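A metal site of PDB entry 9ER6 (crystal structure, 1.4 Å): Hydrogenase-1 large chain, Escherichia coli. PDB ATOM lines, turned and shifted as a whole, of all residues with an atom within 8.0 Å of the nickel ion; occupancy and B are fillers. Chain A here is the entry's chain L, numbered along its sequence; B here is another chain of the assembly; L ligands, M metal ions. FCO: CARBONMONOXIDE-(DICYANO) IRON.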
ATOM      1  N   GLU A  28     -25.932  24.126  -0.778  1.00  0.00           N
ATOM      2  CA  GLU A  28     -24.987  24.045   0.322  1.00  0.00           C
ATOM      3  C   GLU A  28     -25.219  22.727   1.063  1.00  0.00           C
ATOM      4  O   GLU A  28     -26.364  22.431   1.404  1.00  0.00           O
ATOM      5  CB  GLU A  28     -25.140  25.260   1.253  1.00  0.00           C
ATOM      6  CG  GLU A  28     -24.016  25.337   2.262  1.00  0.00           C
ATOM      7  CD  GLU A  28     -24.064  24.237   3.301  1.00  0.00           C
ATOM      8  OE1 GLU A  28     -25.207  23.836   3.623  1.00  0.00           O
ATOM      9  OE2 GLU A  28     -23.000  23.794   3.765  1.00  0.00           O
ATOM     10  N   ARG A  54     -23.979  18.397  12.823  1.00  0.00           N
ATOM     11  CA  ARG A  54     -22.785  18.812  13.544  1.00  0.00           C
ATOM     12  C   ARG A  54     -23.034  19.062  15.029  1.00  0.00           C
ATOM     13  O   ARG A  54     -22.146  18.765  15.835  1.00  0.00           O
ATOM     14  CB  ARG A  54     -22.154  20.060  12.899  1.00  0.00           C
ATOM     15  CG  ARG A  54     -21.488  19.771  11.573  1.00  0.00           C
ATOM     16  CD  ARG A  54     -21.122  20.989  10.775  1.00  0.00           C
ATOM     17  NE  ARG A  54     -22.301  21.727  10.326  1.00  0.00           N
ATOM     18  CZ  ARG A  54     -22.399  23.036  10.213  1.00  0.00           C
ATOM     19  NH1 ARG A  54     -21.333  23.816  10.257  1.00  0.00           N
ATOM     20  NH2 ARG A  54     -23.594  23.571  10.054  1.00  0.00           N
ATOM     21  N   GLU A  73     -21.931  31.528  13.707  1.00  0.00           N
ATOM     22  CA  GLU A  73     -21.668  32.013  12.361  1.00  0.00           C
ATOM     23  C   GLU A  73     -21.265  30.835  11.468  1.00  0.00           C
ATOM     24  O   GLU A  73     -21.678  30.765  10.320  1.00  0.00           O
ATOM     25  CB  GLU A  73     -20.593  33.098  12.300  1.00  0.00           C
ATOM     26  CG  GLU A  73     -20.616  33.838  10.983  1.00  0.00           C
ATOM     27  CD  GLU A  73     -19.788  35.110  10.931  1.00  0.00           C
ATOM     28  OE1 GLU A  73     -18.643  35.070  11.429  1.00  0.00           O
ATOM     29  OE2 GLU A  73     -20.276  36.100  10.370  1.00  0.00           O
ATOM     30  N   ILE A  75     -22.440  27.919  11.440  1.00  0.00           N
ATOM     31  CA  ILE A  75     -23.534  27.103  10.924  1.00  0.00           C
ATOM     32  C   ILE A  75     -23.481  27.114   9.401  1.00  0.00           C
ATOM     33  O   ILE A  75     -23.719  26.099   8.790  1.00  0.00           O
ATOM     34  CB  ILE A  75     -24.882  27.584  11.484  1.00  0.00           C
ATOM     35  CG1 ILE A  75     -25.000  27.249  12.965  1.00  0.00           C
ATOM     36  CG2 ILE A  75     -26.012  26.962  10.690  1.00  0.00           C
ATOM     37  CD1 ILE A  75     -26.190  27.866  13.650  1.00  0.00           C
ATOM     38  N   CYS A  76     -23.015  28.230   8.786  1.00  0.00           N
ATOM     39  CA  CYS A  76     -23.094  28.297   7.340  1.00  0.00           C
ATOM     40  C   CYS A  76     -22.163  29.369   6.760  1.00  0.00           C
ATOM     41  O   CYS A  76     -22.198  30.487   7.231  1.00  0.00           O
ATOM     42  CB  CYS A  76     -24.512  28.618   6.914  1.00  0.00           C
ATOM     43  SG  CYS A  76     -24.654  28.379   5.124  1.00  0.00           S
ATOM     44  N   GLY A  77     -21.375  28.986   5.739  1.00  0.00           N
ATOM     45  CA  GLY A  77     -20.439  29.866   5.056  1.00  0.00           C
ATOM     46  C   GLY A  77     -21.059  30.472   3.797  1.00  0.00           C
ATOM     47  O   GLY A  77     -20.455  31.356   3.192  1.00  0.00           O
ATOM     48  N   VAL A  78     -22.257  29.992   3.441  1.00  0.00           N
ATOM     49  CA  VAL A  78     -23.016  30.544   2.323  1.00  0.00           C
ATOM     50  C   VAL A  78     -23.825  31.732   2.833  1.00  0.00           C
ATOM     51  O   VAL A  78     -23.572  32.854   2.394  1.00  0.00           O
ATOM     52  CB  VAL A  78     -23.887  29.503   1.614  1.00  0.00           C
ATOM     53  CG1 VAL A  78     -24.716  30.160   0.516  1.00  0.00           C
ATOM     54  CG2 VAL A  78     -23.051  28.369   1.061  1.00  0.00           C
ATOM     55  N   CYS A  79     -24.700  31.506   3.828  1.00  0.00           N
ATOM     56  CA  CYS A  79     -25.405  32.610   4.456  1.00  0.00           C
ATOM     57  C   CYS A  79     -24.534  33.142   5.592  1.00  0.00           C
ATOM     58  O   CYS A  79     -24.973  33.341   6.729  1.00  0.00           O
ATOM     59  CB  CYS A  79     -26.822  32.226   4.887  1.00  0.00           C
ATOM     60  SG  CYS A  79     -26.947  30.835   6.034  1.00  0.00           S
ATOM     61  N   THR A  80     -23.268  33.426   5.247  1.00  0.00           N
ATOM     62  CA  THR A  80     -22.255  33.815   6.230  1.00  0.00           C
ATOM     63  C   THR A  80     -22.615  35.191   6.786  1.00  0.00           C
ATOM     64  O   THR A  80     -22.786  36.177   6.046  1.00  0.00           O
ATOM     65  CB  THR A  80     -20.830  33.841   5.638  1.00  0.00           C
ATOM     66  OG1 THR A  80     -19.918  34.182   6.671  1.00  0.00           O
ATOM     67  CG2 THR A  80     -20.644  34.841   4.527  1.00  0.00           C
ATOM     68  N   VAL A  82     -25.331  35.769   8.831  1.00  0.00           N
ATOM     69  CA  VAL A  82     -26.717  35.917   9.264  1.00  0.00           C
ATOM     70  C   VAL A  82     -26.896  35.304  10.641  1.00  0.00           C
ATOM     71  O   VAL A  82     -27.653  35.835  11.469  1.00  0.00           O
ATOM     72  CB  VAL A  82     -27.752  35.389   8.241  1.00  0.00           C
ATOM     73  CG1 VAL A  82     -27.817  33.881   8.203  1.00  0.00           C
ATOM     74  CG2 VAL A  82     -29.122  35.975   8.582  1.00  0.00           C
ATOM     75  N   HIS A  83     -26.202  34.215  10.914  1.00  0.00           N
ATOM     76  CA  HIS A  83     -26.249  33.580  12.227  1.00  0.00           C
ATOM     77  C   HIS A  83     -25.531  34.420  13.269  1.00  0.00           C
ATOM     78  O   HIS A  83     -25.967  34.433  14.419  1.00  0.00           O
ATOM     79  CB  HIS A  83     -25.715  32.153  12.190  1.00  0.00           C
ATOM     80  CG  HIS A  83     -26.601  31.235  11.436  1.00  0.00           C
ATOM     81  ND1 HIS A  83     -27.794  30.779  11.945  1.00  0.00           N
ATOM     82  CD2 HIS A  83     -26.429  30.662  10.208  1.00  0.00           C
ATOM     83  CE1 HIS A  83     -28.352  29.961  11.046  1.00  0.00           C
ATOM     84  NE2 HIS A  83     -27.555  29.908   9.947  1.00  0.00           N
ATOM     85  N   LEU A 114     -25.164  40.581   2.249  1.00  0.00           N
ATOM     86  CA  LEU A 114     -25.353  39.150   2.184  1.00  0.00           C
ATOM     87  C   LEU A 114     -26.504  38.778   1.244  1.00  0.00           C
ATOM     88  O   LEU A 114     -26.362  37.859   0.450  1.00  0.00           O
ATOM     89  CB  LEU A 114     -25.555  38.544   3.566  1.00  0.00           C
ATOM     90  CG  LEU A 114     -25.805  37.033   3.519  1.00  0.00           C
ATOM     91  CD1 LEU A 114     -24.595  36.266   2.963  1.00  0.00           C
ATOM     92  CD2 LEU A 114     -26.171  36.539   4.880  1.00  0.00           C
ATOM     93  N   ASP A 118     -25.582  36.492  -1.859  1.00  0.00           N
ATOM     94  CA  ASP A 118     -26.101  35.132  -1.769  1.00  0.00           C
ATOM     95  C   ASP A 118     -27.083  34.889  -2.921  1.00  0.00           C
ATOM     96  O   ASP A 118     -27.029  33.878  -3.627  1.00  0.00           O
ATOM     97  CB  ASP A 118     -26.710  34.936  -0.385  1.00  0.00           C
ATOM     98  CG  ASP A 118     -26.923  33.491   0.008  1.00  0.00           C
ATOM     99  OD1 ASP A 118     -27.209  32.677  -0.883  1.00  0.00           O
ATOM    100  OD2 ASP A 118     -26.818  33.203   1.247  1.00  0.00           O
ATOM    101  N   ALA A 507     -33.074  35.627   6.819  1.00  0.00           N
ATOM    102  CA  ALA A 507     -31.871  35.245   6.112  1.00  0.00           C
ATOM    103  C   ALA A 507     -32.214  35.162   4.620  1.00  0.00           C
ATOM    104  O   ALA A 507     -33.398  35.135   4.275  1.00  0.00           O
ATOM    105  CB  ALA A 507     -31.377  33.937   6.665  1.00  0.00           C
ATOM    106  N   PRO A 508     -31.238  35.052   3.696  1.00  0.00           N
ATOM    107  CA  PRO A 508     -31.559  34.865   2.271  1.00  0.00           C
ATOM    108  C   PRO A 508     -32.646  33.814   2.015  1.00  0.00           C
ATOM    109  O   PRO A 508     -33.430  33.964   1.098  1.00  0.00           O
ATOM    110  CB  PRO A 508     -30.194  34.566   1.645  1.00  0.00           C
ATOM    111  CG  PRO A 508     -29.237  35.348   2.552  1.00  0.00           C
ATOM    112  CD  PRO A 508     -29.782  35.203   3.941  1.00  0.00           C
ATOM    113  N   ARG A 509     -32.656  32.710   2.787  1.00  0.00           N
ATOM    114  CA  ARG A 509     -33.539  31.585   2.523  1.00  0.00           C
ATOM    115  C   ARG A 509     -34.848  31.619   3.319  1.00  0.00           C
ATOM    116  O   ARG A 509     -35.687  30.732   3.110  1.00  0.00           O
ATOM    117  CB  ARG A 509     -32.772  30.285   2.781  1.00  0.00           C
ATOM    118  CG  ARG A 509     -31.634  30.104   1.793  1.00  0.00           C
ATOM    119  CD  ARG A 509     -30.558  29.108   2.144  1.00  0.00           C
ATOM    120  NE  ARG A 509     -29.596  29.164   1.050  1.00  0.00           N
ATOM    121  CZ  ARG A 509     -28.612  30.039   0.923  1.00  0.00           C
ATOM    122  NH1 ARG A 509     -28.408  30.978   1.833  1.00  0.00           N
ATOM    123  NH2 ARG A 509     -27.879  30.007  -0.177  1.00  0.00           N
ATOM    124  N   VAL A 530     -33.934  27.339  11.570  1.00  0.00           N
ATOM    125  CA  VAL A 530     -33.315  28.028  10.453  1.00  0.00           C
ATOM    126  C   VAL A 530     -34.197  27.856   9.217  1.00  0.00           C
ATOM    127  O   VAL A 530     -35.036  26.945   9.169  1.00  0.00           O
ATOM    128  CB  VAL A 530     -31.899  27.438  10.302  1.00  0.00           C
ATOM    129  CG1 VAL A 530     -31.057  28.099   9.241  1.00  0.00           C
ATOM    130  CG2 VAL A 530     -31.186  27.530  11.638  1.00  0.00           C
ATOM    131  N   PRO A 531     -34.161  28.769   8.216  1.00  0.00           N
ATOM    132  CA  PRO A 531     -35.154  28.704   7.157  1.00  0.00           C
ATOM    133  C   PRO A 531     -35.220  27.342   6.487  1.00  0.00           C
ATOM    134  O   PRO A 531     -36.340  26.871   6.235  1.00  0.00           O
ATOM    135  CB  PRO A 531     -34.781  29.827   6.186  1.00  0.00           C
ATOM    136  CG  PRO A 531     -33.572  30.497   6.795  1.00  0.00           C
ATOM    137  CD  PRO A 531     -33.463  30.049   8.225  1.00  0.00           C
ATOM    138  N   THR A 532     -34.070  26.738   6.135  1.00  0.00           N
ATOM    139  CA  THR A 532     -34.126  25.461   5.461  1.00  0.00           C
ATOM    140  C   THR A 532     -34.674  24.379   6.416  1.00  0.00           C
ATOM    141  O   THR A 532     -35.150  23.345   5.948  1.00  0.00           O
ATOM    142  CB  THR A 532     -32.791  25.123   4.768  1.00  0.00           C
ATOM    143  OG1 THR A 532     -32.508  26.138   3.797  1.00  0.00           O
ATOM    144  CG2 THR A 532     -32.790  23.801   4.036  1.00  0.00           C
ATOM    145  N   ASP A 574     -33.472  27.260  -2.784  1.00  0.00           N
ATOM    146  CA  ASP A 574     -32.114  27.627  -2.391  1.00  0.00           C
ATOM    147  C   ASP A 574     -31.750  26.839  -1.122  1.00  0.00           C
ATOM    148  O   ASP A 574     -31.512  27.415  -0.055  1.00  0.00           O
ATOM    149  CB  ASP A 574     -32.022  29.134  -2.211  1.00  0.00           C
ATOM    150  CG  ASP A 574     -30.658  29.698  -1.900  1.00  0.00           C
ATOM    151  OD1 ASP A 574     -29.653  28.954  -1.973  1.00  0.00           O
ATOM    152  OD2 ASP A 574     -30.639  30.899  -1.504  1.00  0.00           O
ATOM    153  N   PRO A 575     -31.743  25.495  -1.155  1.00  0.00           N
ATOM    154  CA  PRO A 575     -31.497  24.709   0.052  1.00  0.00           C
ATOM    155  C   PRO A 575     -30.118  24.971   0.663  1.00  0.00           C
ATOM    156  O   PRO A 575     -29.095  24.946  -0.029  1.00  0.00           O
ATOM    157  CB  PRO A 575     -31.582  23.247  -0.395  1.00  0.00           C
ATOM    158  CG  PRO A 575     -32.395  23.326  -1.671  1.00  0.00           C
ATOM    159  CD  PRO A 575     -31.997  24.635  -2.325  1.00  0.00           C
ATOM    160  N   CYS A 576     -30.118  25.179   1.981  1.00  0.00           N
ATOM    161  CA  CYS A 576     -28.886  25.272   2.759  1.00  0.00           C
ATOM    162  C   CYS A 576     -28.933  24.198   3.849  1.00  0.00           C
ATOM    163  O   CYS A 576     -29.595  24.342   4.875  1.00  0.00           O
ATOM    164  CB  CYS A 576     -28.731  26.649   3.350  1.00  0.00           C
ATOM    165  SG  CYS A 576     -27.039  26.901   3.974  1.00  0.00           S
ATOM    166  N   LEU A 577     -28.267  23.085   3.589  1.00  0.00           N
ATOM    167  CA  LEU A 577     -28.436  21.917   4.428  1.00  0.00           C
ATOM    168  C   LEU A 577     -27.661  22.027   5.729  1.00  0.00           C
ATOM    169  O   LEU A 577     -28.137  21.529   6.771  1.00  0.00           O
ATOM    170  CB  LEU A 577     -28.110  20.655   3.627  1.00  0.00           C
ATOM    171  CG  LEU A 577     -29.306  20.125   2.813  1.00  0.00           C
ATOM    172  CD1 LEU A 577     -30.391  19.500   3.672  1.00  0.00           C
ATOM    173  CD2 LEU A 577     -29.905  21.218   1.927  1.00  0.00           C
ATOM    174  N   ALA A 578     -26.478  22.658   5.703  1.00  0.00           N
ATOM    175  CA  ALA A 578     -25.742  22.891   6.952  1.00  0.00           C
ATOM    176  C   ALA A 578     -26.548  23.782   7.886  1.00  0.00           C
ATOM    177  O   ALA A 578     -26.601  23.572   9.099  1.00  0.00           O
ATOM    178  CB  ALA A 578     -24.382  23.533   6.678  1.00  0.00           C
ATOM    179  N   CYS A 579     -27.153  24.828   7.317  1.00  0.00           N
ATOM    180  CA  CYS A 579     -28.132  25.631   8.038  1.00  0.00           C
ATOM    181  C   CYS A 579     -29.228  24.766   8.653  1.00  0.00           C
ATOM    182  O   CYS A 579     -29.562  24.971   9.824  1.00  0.00           O
ATOM    183  CB  CYS A 579     -28.801  26.674   7.139  1.00  0.00           C
ATOM    184  SG  CYS A 579     -27.908  28.243   7.103  1.00  0.00           S
ATOM    185  N   SER A 580     -29.816  23.892   7.838  1.00  0.00           N
ATOM    186  CA  SER A 580     -31.038  23.189   8.218  1.00  0.00           C
ATOM    187  C   SER A 580     -30.835  22.315   9.455  1.00  0.00           C
ATOM    188  O   SER A 580     -31.777  22.179  10.240  1.00  0.00           O
ATOM    189  CB  SER A 580     -31.598  22.371   7.082  1.00  0.00           C
ATOM    190  OG  SER A 580     -30.838  21.195   6.836  1.00  0.00           O
ATOM    191  N   CYS B  17     -19.443  23.886   6.684  1.00  0.00           N
ATOM    192  CA  CYS B  17     -20.367  24.975   6.472  1.00  0.00           C
ATOM    193  C   CYS B  17     -20.252  25.541   5.042  1.00  0.00           C
ATOM    194  O   CYS B  17     -21.036  26.404   4.725  1.00  0.00           O
ATOM    195  CB  CYS B  17     -20.151  26.077   7.506  1.00  0.00           C
ATOM    196  SG  CYS B  17     -18.824  27.251   7.095  1.00  0.00           S
ATOM    197  N   THR B  18     -19.288  25.075   4.247  1.00  0.00           N
ATOM    198  CA  THR B  18     -19.041  25.505   2.873  1.00  0.00           C
ATOM    199  C   THR B  18     -18.290  26.847   2.795  1.00  0.00           C
ATOM    200  O   THR B  18     -18.159  27.449   1.694  1.00  0.00           O
ATOM    201  CB  THR B  18     -20.317  25.458   2.019  1.00  0.00           C
ATOM    202  OG1 THR B  18     -21.029  24.237   2.312  1.00  0.00           O
ATOM    203  CG2 THR B  18     -20.009  25.491   0.541  1.00  0.00           C
HETATM  204 FE   FCO L   1     -29.026  29.857   6.033  1.00  0.00          FE
HETATM  205  C1  FCO L   1     -30.523  28.759   5.723  1.00  0.00           C
HETATM  206  N1  FCO L   1     -31.452  28.046   5.540  1.00  0.00           N
HETATM  207  C2  FCO L   1     -29.781  31.139   4.923  1.00  0.00           C
HETATM  208  N2  FCO L   1     -30.261  31.914   4.169  1.00  0.00           N
HETATM  209  C3  FCO L   1     -29.764  30.679   7.427  1.00  0.00           C
HETATM  210  O3  FCO L   1     -30.229  31.252   8.338  1.00  0.00           O
HETATM  211 NI    NI M   1     -26.830  28.681   5.034  1.00  0.00          NI
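An iron atom (FE) of the ligand is bound by the side-chain sulfur (SG) of Cys 579, at 2.2 Å. An iron atom (FE) of the ligand is bound by the side-chain sulfur (SG) of Cys 79 (2.3 Å). The backbone NH of Arg 509 lies within hydrogen-bond range of a nitrogen (N2) of the ligand. A nitrogen (N2) of the ligand is in hydrogen-bond range of the guanidinium group of Arg 509, at 3.1 Å. NE2 of His 83 sits at hydrogen-bond distance from O3 of the ligand, at 3.4 Å. N1 of the ligand lies within hydrogen-bond range of N of Thr 532 (3.0 Å). OG1 of Thr 532 is in hydrogen-bond range of N1 of the ligand, at 2.8 Å.
The side-chain sulfur of Cys 576 lies close to the side-chain carboxylate of Glu 28. N of Cys 576 is in hydrogen-bond range of OG1 of Thr 532, 3.2 Å away. The side-chain sulfur (SG) of Cys 76 lies close to the backbone NH (N) of Val 78, at 3.3 Å. The side-chain sulfur (SG) of Cys 579 sits close to a ring nitrogen (NE2) of His 83, at 3.3 Å.
Four residues have an atom within 4 Å of the nickel ion: Cys 76, Cys 79, Cys 576 and Cys 579. The nearest printed residue that does not touch the nickel ion is Arg 509 (4.2 Å).
The nickel ion is bound by SG of Cys 576 (2.1 Å), SG of Cys 76 (2.2 Å), SG of Cys 579 (2.4 Å) and SG of Cys 79 (2.4 Å). The nickel ion has four donor atoms within binding distance.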
